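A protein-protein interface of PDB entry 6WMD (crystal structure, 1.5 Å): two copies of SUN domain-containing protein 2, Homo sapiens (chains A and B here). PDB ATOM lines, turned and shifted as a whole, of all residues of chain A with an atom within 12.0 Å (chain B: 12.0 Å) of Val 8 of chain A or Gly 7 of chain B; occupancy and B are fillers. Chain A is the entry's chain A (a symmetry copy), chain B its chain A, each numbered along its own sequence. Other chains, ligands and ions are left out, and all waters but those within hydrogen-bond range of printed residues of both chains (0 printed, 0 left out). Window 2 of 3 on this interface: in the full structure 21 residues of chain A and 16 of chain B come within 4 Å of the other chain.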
ATOM      1  N   GLY A   7      11.269  -2.241 -25.498  1.00  0.00           N
ATOM      2  CA  GLY A   7      10.326  -3.341 -25.419  1.00  0.00           C
ATOM      3  C   GLY A   7       9.438  -3.294 -24.190  1.00  0.00           C
ATOM      4  O   GLY A   7       8.706  -2.328 -23.977  1.00  0.00           O
ATOM      5  N   VAL A   8       9.497  -4.347 -23.381  1.00  0.00           N
ATOM      6  CA  VAL A   8       8.709  -4.445 -22.161  1.00  0.00           C
ATOM      7  C   VAL A   8       9.652  -4.457 -20.971  1.00  0.00           C
ATOM      8  O   VAL A   8      10.805  -4.890 -21.067  1.00  0.00           O
ATOM      9  CB  VAL A   8       7.818  -5.704 -22.152  1.00  0.00           C
ATOM     10  CG1 VAL A   8       6.569  -5.476 -22.982  1.00  0.00           C
ATOM     11  CG2 VAL A   8       8.602  -6.900 -22.659  1.00  0.00           C
ATOM     12  N   THR A   9       9.149  -3.985 -19.839  1.00  0.00           N
ATOM     13  CA  THR A   9       9.921  -4.011 -18.609  1.00  0.00           C
ATOM     14  C   THR A   9       9.732  -5.347 -17.898  1.00  0.00           C
ATOM     15  O   THR A   9       8.781  -6.091 -18.155  1.00  0.00           O
ATOM     16  CB  THR A   9       9.480  -2.876 -17.691  1.00  0.00           C
ATOM     17  OG1 THR A   9       8.113  -3.074 -17.316  1.00  0.00           O
ATOM     18  CG2 THR A   9       9.620  -1.532 -18.393  1.00  0.00           C
ATOM     19  N   GLU A  10      10.668  -5.650 -16.995  1.00  0.00           N
ATOM     20  CA  GLU A  10      10.543  -6.850 -16.173  1.00  0.00           C
ATOM     21  C   GLU A  10       9.243  -6.840 -15.382  1.00  0.00           C
ATOM     22  O   GLU A  10       8.581  -7.877 -15.247  1.00  0.00           O
ATOM     23  CB  GLU A  10      11.739  -6.958 -15.227  1.00  0.00           C
ATOM     24  CG  GLU A  10      12.129  -8.382 -14.879  1.00  0.00           C
ATOM     25  CD  GLU A  10      13.041  -8.454 -13.669  1.00  0.00           C
ATOM     26  OE1 GLU A  10      13.818  -7.502 -13.448  1.00  0.00           O
ATOM     27  OE2 GLU A  10      12.976  -9.459 -12.935  1.00  0.00           O
ATOM     28  N   GLU A  11       8.858  -5.675 -14.859  1.00  0.00           N
ATOM     29  CA  GLU A  11       7.611  -5.569 -14.111  1.00  0.00           C
ATOM     30  C   GLU A  11       6.416  -5.909 -14.989  1.00  0.00           C
ATOM     31  O   GLU A  11       5.483  -6.592 -14.545  1.00  0.00           O
ATOM     32  CB  GLU A  11       7.473  -4.165 -13.521  1.00  0.00           C
ATOM     33  CG  GLU A  11       8.719  -3.677 -12.789  1.00  0.00           C
ATOM     34  CD  GLU A  11       9.727  -3.004 -13.709  1.00  0.00           C
ATOM     35  OE1 GLU A  11      10.942  -3.091 -13.433  1.00  0.00           O
ATOM     36  OE2 GLU A  11       9.301  -2.377 -14.698  1.00  0.00           O
ATOM     37  N   GLN A  12       6.431  -5.451 -16.244  1.00  0.00           N
ATOM     38  CA  GLN A  12       5.358  -5.790 -17.172  1.00  0.00           C
ATOM     39  C   GLN A  12       5.296  -7.291 -17.429  1.00  0.00           C
ATOM     40  O   GLN A  12       4.205  -7.865 -17.521  1.00  0.00           O
ATOM     41  CB  GLN A  12       5.529  -5.020 -18.483  1.00  0.00           C
ATOM     42  CG  GLN A  12       4.994  -3.594 -18.438  1.00  0.00           C
ATOM     43  CD  GLN A  12       5.307  -2.803 -19.697  1.00  0.00           C
ATOM     44  OE1 GLN A  12       6.411  -2.885 -20.243  1.00  0.00           O
ATOM     45  NE2 GLN A  12       4.334  -2.025 -20.160  1.00  0.00           N
ATOM     46  N   VAL A  13       6.454  -7.951 -17.547  1.00  0.00           N
ATOM     47  CA  VAL A  13       6.451  -9.401 -17.752  1.00  0.00           C
ATOM     48  C   VAL A  13       5.827 -10.109 -16.557  1.00  0.00           C
ATOM     49  O   VAL A  13       4.983 -10.996 -16.713  1.00  0.00           O
ATOM     50  CB  VAL A  13       7.867  -9.932 -18.042  1.00  0.00           C
ATOM     51  CG1 VAL A  13       7.833 -11.451 -18.198  1.00  0.00           C
ATOM     52  CG2 VAL A  13       8.432  -9.290 -19.294  1.00  0.00           C
ATOM     53  N   HIS A  14       6.242  -9.738 -15.343  1.00  0.00           N
ATOM     54  CA  HIS A  14       5.680 -10.378 -14.157  1.00  0.00           C
ATOM     55  C   HIS A  14       4.176 -10.178 -14.094  1.00  0.00           C
ATOM     56  O   HIS A  14       3.434 -11.097 -13.722  1.00  0.00           O
ATOM     57  CB  HIS A  14       6.341  -9.810 -12.902  1.00  0.00           C
ATOM     58  CG  HIS A  14       7.701 -10.368 -12.639  1.00  0.00           C
ATOM     59  ND1 HIS A  14       7.911 -11.688 -12.300  1.00  0.00           N
ATOM     60  CD2 HIS A  14       8.922  -9.787 -12.669  1.00  0.00           C
ATOM     61  CE1 HIS A  14       9.206 -11.894 -12.136  1.00  0.00           C
ATOM     62  NE2 HIS A  14       9.841 -10.758 -12.354  1.00  0.00           N
ATOM     63  N   HIS A  15       3.710  -8.986 -14.477  1.00  0.00           N
ATOM     64  CA  HIS A  15       2.283  -8.692 -14.466  1.00  0.00           C
ATOM     65  C   HIS A  15       1.533  -9.575 -15.459  1.00  0.00           C
ATOM     66  O   HIS A  15       0.487 -10.145 -15.132  1.00  0.00           O
ATOM     67  CB  HIS A  15       2.076  -7.211 -14.788  1.00  0.00           C
ATOM     68  CG  HIS A  15       0.645  -6.779 -14.747  1.00  0.00           C
ATOM     69  ND1 HIS A  15      -0.022  -6.534 -13.567  1.00  0.00           N
ATOM     70  CD2 HIS A  15      -0.249  -6.560 -15.739  1.00  0.00           C
ATOM     71  CE1 HIS A  15      -1.264  -6.172 -13.834  1.00  0.00           C
ATOM     72  NE2 HIS A  15      -1.429  -6.180 -15.144  1.00  0.00           N
ATOM     73  N   ILE A  16       2.051  -9.691 -16.686  1.00  0.00           N
ATOM     74  CA  ILE A  16       1.411 -10.527 -17.702  1.00  0.00           C
ATOM     75  C   ILE A  16       1.326 -11.974 -17.230  1.00  0.00           C
ATOM     76  O   ILE A  16       0.290 -12.639 -17.371  1.00  0.00           O
ATOM     77  CB  ILE A  16       2.161 -10.394 -19.041  1.00  0.00           C
ATOM     78  CG1 ILE A  16       1.936  -8.998 -19.628  1.00  0.00           C
ATOM     79  CG2 ILE A  16       1.714 -11.460 -20.022  1.00  0.00           C
ATOM     80  CD1 ILE A  16       2.913  -8.619 -20.741  1.00  0.00           C
ATOM     81  N   VAL A  17       2.417 -12.482 -16.657  1.00  0.00           N
ATOM     82  CA  VAL A  17       2.460 -13.868 -16.202  1.00  0.00           C
ATOM     83  C   VAL A  17       1.481 -14.086 -15.056  1.00  0.00           C
ATOM     84  O   VAL A  17       0.718 -15.063 -15.045  1.00  0.00           O
ATOM     85  CB  VAL A  17       3.899 -14.232 -15.797  1.00  0.00           C
ATOM     86  CG1 VAL A  17       3.933 -15.589 -15.112  1.00  0.00           C
ATOM     87  CG2 VAL A  17       4.824 -14.206 -17.016  1.00  0.00           C
ATOM     88  N   GLY B   7      14.849  -3.280 -22.516  1.00  0.00           N
ATOM     89  CA  GLY B   7      13.902  -3.980 -21.670  1.00  0.00           C
ATOM     90  C   GLY B   7      14.414  -5.310 -21.152  1.00  0.00           C
ATOM     91  O   GLY B   7      15.441  -5.373 -20.476  1.00  0.00           O
ATOM     92  N   VAL B   8      13.691  -6.380 -21.467  1.00  0.00           N
ATOM     93  CA  VAL B   8      14.058  -7.725 -21.049  1.00  0.00           C
ATOM     94  C   VAL B   8      14.386  -8.548 -22.283  1.00  0.00           C
ATOM     95  O   VAL B   8      13.874  -8.298 -23.379  1.00  0.00           O
ATOM     96  CB  VAL B   8      12.935  -8.403 -20.238  1.00  0.00           C
ATOM     97  CG1 VAL B   8      12.950  -7.915 -18.802  1.00  0.00           C
ATOM     98  CG2 VAL B   8      11.591  -8.140 -20.889  1.00  0.00           C
ATOM     99  N   THR B   9      15.241  -9.544 -22.097  1.00  0.00           N
ATOM    100  CA  THR B   9      15.579 -10.452 -23.178  1.00  0.00           C
ATOM    101  C   THR B   9      14.573 -11.597 -23.237  1.00  0.00           C
ATOM    102  O   THR B   9      13.849 -11.875 -22.277  1.00  0.00           O
ATOM    103  CB  THR B   9      16.981 -11.014 -22.971  1.00  0.00           C
ATOM    104  OG1 THR B   9      17.008 -11.787 -21.766  1.00  0.00           O
ATOM    105  CG2 THR B   9      18.001  -9.886 -22.867  1.00  0.00           C
ATOM    106  N   GLU B  10      14.532 -12.261 -24.394  1.00  0.00           N
ATOM    107  CA  GLU B  10      13.687 -13.442 -24.541  1.00  0.00           C
ATOM    108  C   GLU B  10      14.043 -14.503 -23.510  1.00  0.00           C
ATOM    109  O   GLU B  10      13.156 -15.155 -22.945  1.00  0.00           O
ATOM    110  CB  GLU B  10      13.826 -14.008 -25.954  1.00  0.00           C
ATOM    111  CG  GLU B  10      12.578 -14.700 -26.472  1.00  0.00           C
ATOM    112  CD  GLU B  10      12.858 -15.568 -27.684  1.00  0.00           C
ATOM    113  OE1 GLU B  10      13.777 -15.234 -28.459  1.00  0.00           O
ATOM    114  OE2 GLU B  10      12.163 -16.589 -27.857  1.00  0.00           O
ATOM    115  N   GLU B  11      15.339 -14.682 -23.245  1.00  0.00           N
ATOM    116  CA  GLU B  11      15.769 -15.658 -22.250  1.00  0.00           C
ATOM    117  C   GLU B  11      15.232 -15.305 -20.871  1.00  0.00           C
ATOM    118  O   GLU B  11      14.797 -16.189 -20.120  1.00  0.00           O
ATOM    119  CB  GLU B  11      17.295 -15.750 -22.234  1.00  0.00           C
ATOM    120  CG  GLU B  11      17.920 -15.907 -23.616  1.00  0.00           C
ATOM    121  CD  GLU B  11      18.179 -14.578 -24.309  1.00  0.00           C
ATOM    122  OE1 GLU B  11      18.113 -14.528 -25.556  1.00  0.00           O
ATOM    123  OE2 GLU B  11      18.464 -13.589 -23.606  1.00  0.00           O
ATOM    124  N   GLN B  12      15.240 -14.015 -20.525  1.00  0.00           N
ATOM    125  CA  GLN B  12      14.679 -13.583 -19.249  1.00  0.00           C
ATOM    126  C   GLN B  12      13.185 -13.877 -19.168  1.00  0.00           C
ATOM    127  O   GLN B  12      12.686 -14.285 -18.114  1.00  0.00           O
ATOM    128  CB  GLN B  12      14.953 -12.095 -19.027  1.00  0.00           C
ATOM    129  CG  GLN B  12      16.343 -11.796 -18.478  1.00  0.00           C
ATOM    130  CD  GLN B  12      16.645 -10.308 -18.407  1.00  0.00           C
ATOM    131  OE1 GLN B  12      16.315  -9.546 -19.319  1.00  0.00           O
ATOM    132  NE2 GLN B  12      17.282  -9.889 -17.318  1.00  0.00           N
ATOM    133  N   VAL B  13      12.452 -13.683 -20.270  1.00  0.00           N
ATOM    134  CA  VAL B  13      11.020 -13.991 -20.258  1.00  0.00           C
ATOM    135  C   VAL B  13      10.796 -15.477 -20.011  1.00  0.00           C
ATOM    136  O   VAL B  13       9.964 -15.866 -19.188  1.00  0.00           O
ATOM    137  CB  VAL B  13      10.334 -13.527 -21.556  1.00  0.00           C
ATOM    138  CG1 VAL B  13       8.856 -13.911 -21.532  1.00  0.00           C
ATOM    139  CG2 VAL B  13      10.483 -12.029 -21.733  1.00  0.00           C
ATOM    140  N   HIS B  14      11.524 -16.332 -20.733  1.00  0.00           N
ATOM    141  CA  HIS B  14      11.355 -17.770 -20.541  1.00  0.00           C
ATOM    142  C   HIS B  14      11.661 -18.165 -19.107  1.00  0.00           C
ATOM    143  O   HIS B  14      10.970 -19.013 -18.526  1.00  0.00           O
ATOM    144  CB  HIS B  14      12.267 -18.529 -21.503  1.00  0.00           C
ATOM    145  CG  HIS B  14      11.745 -18.589 -22.900  1.00  0.00           C
ATOM    146  ND1 HIS B  14      10.604 -19.285 -23.239  1.00  0.00           N
ATOM    147  CD2 HIS B  14      12.202 -18.034 -24.046  1.00  0.00           C
ATOM    148  CE1 HIS B  14      10.382 -19.153 -24.536  1.00  0.00           C
ATOM    149  NE2 HIS B  14      11.337 -18.400 -25.047  1.00  0.00           N
ATOM    150  N   ILE B  16      11.386 -16.238 -16.334  1.00  0.00           N
ATOM    151  CA  ILE B  16      10.301 -15.779 -15.466  1.00  0.00           C
ATOM    152  C   ILE B  16       9.104 -16.719 -15.563  1.00  0.00           C
ATOM    153  O   ILE B  16       8.498 -17.097 -14.551  1.00  0.00           O
ATOM    154  CB  ILE B  16       9.930 -14.326 -15.815  1.00  0.00           C
ATOM    155  CG1 ILE B  16      11.060 -13.384 -15.390  1.00  0.00           C
ATOM    156  CG2 ILE B  16       8.626 -13.923 -15.150  1.00  0.00           C
ATOM    157  CD1 ILE B  16      10.980 -11.988 -16.010  1.00  0.00           C
ATOM    158  N   VAL B  17       8.749 -17.113 -16.787  1.00  0.00           N
ATOM    159  CA  VAL B  17       7.595 -17.982 -16.999  1.00  0.00           C
ATOM    160  C   VAL B  17       7.837 -19.353 -16.381  1.00  0.00           C
ATOM    161  O   VAL B  17       6.970 -19.900 -15.683  1.00  0.00           O
ATOM    162  CB  VAL B  17       7.297 -18.082 -18.505  1.00  0.00           C
ATOM    163  CG1 VAL B  17       6.249 -19.151 -18.771  1.00  0.00           C
ATOM    164  CG2 VAL B  17       6.855 -16.725 -19.056  1.00  0.00           C
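Gly 7 of chain B touches Val 8 of chain A. Glu 10 of chain A touches Val 8 of chain B (N to CG1, 3.7 Å). Ile 16 of chain B touches Glu 10 of chain A (CD1 to CG, 3.95 Å). Val 8 of chain B touches Val 13 of chain A. CD1 of Ile 16 of chain B touches CG1 of Val 13 of chain A, at 3.9 Å. CG2 of Ile 16 of chain B touches CE1 of His 14 of chain A (3.7 Å). Val 17 of chain A touches Val 17 of chain B (CG2 to CG2, 3.8 Å).
Val 8 of chain A touches two residues of chain B. No residue of chain B comes within 4 Å of Thr 9 of chain A. Of the printed residues of chain B, Glu 10 of chain A touches Val 8 and Ile 16. No residue of chain B comes within 4 Å of Gln 12 of chain A. Printed residues of chain B within 4 Å of Val 17 of chain A: Val 17. Val 8 of chain B touches just these residues of chain A: Val 8, Glu 10 and Val 13. Thr 9 of chain B touches none of the printed residues of chain A. Val 13 of chain B touches none of the printed residues of chain A. His 14 of chain B touches none of the printed residues of chain A. Printed residues of chain A within 4 Å of Ile 16 of chain B: Glu 10, Val 13 and His 14. Of the printed residues of chain A, Val 17 of chain B touches Val 17. The nearest residue of chain B that does not touch Val 8 of chain A is Val 13 of chain B (5.5 Å). The nearest printed residue of chain B that does not touch Val 17 of chain A is Ile 16 of chain B (4.2 Å).
Val 8 of chain A touches its own counterpart, Val 8 of chain B. Glu 10 of chain A touches Val 8 of chain B, but with the chains exchanged Val 8 of chain A does not touch Glu 10 of chain B (8.2 Å). Val 13 of chain A touches Val 8 of chain B, but with the chains exchanged Val 8 of chain A does not touch Val 13 of chain B (5.5 Å). His 14 of chain A touches Ile 16 of chain B, but with the chains exchanged Ile 16 of chain A does not touch His 14 of chain B (11.0 Å). Positions printed for both chains: 7, 8, 9, 10, 11, 12, 13, 14, 16 and 17.
Printed residues of chain A that touch a printed residue of chain B: Val 8, Glu 10, Val 13, His 14 and Val 17. Hydrophobic or aromatic side chains of chain A that line the printed part of chain B: Val 8, Val 13, His 14 and Val 17. Of the 10 printed residues of chain B, 4 touch a printed residue of chain A. Among the printed residues, 8 pairs touch across the chains. Among the printed residues, no Asp or Glu carboxylate lies within 4 Å of a Lys or Arg side-chain nitrogen of the other chain.
The side-chain carboxylate (OE2) of Glu 10 of chain A lies within hydrogen-bond range of a ring nitrogen (NE2) of His 14 of chain A, at 3.4 Å.
The backbone NH of Val 8 of chain B sits at hydrogen-bond distance from the backbone carbonyl oxygen of Val 8 of chain A, at 3.3 Å.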
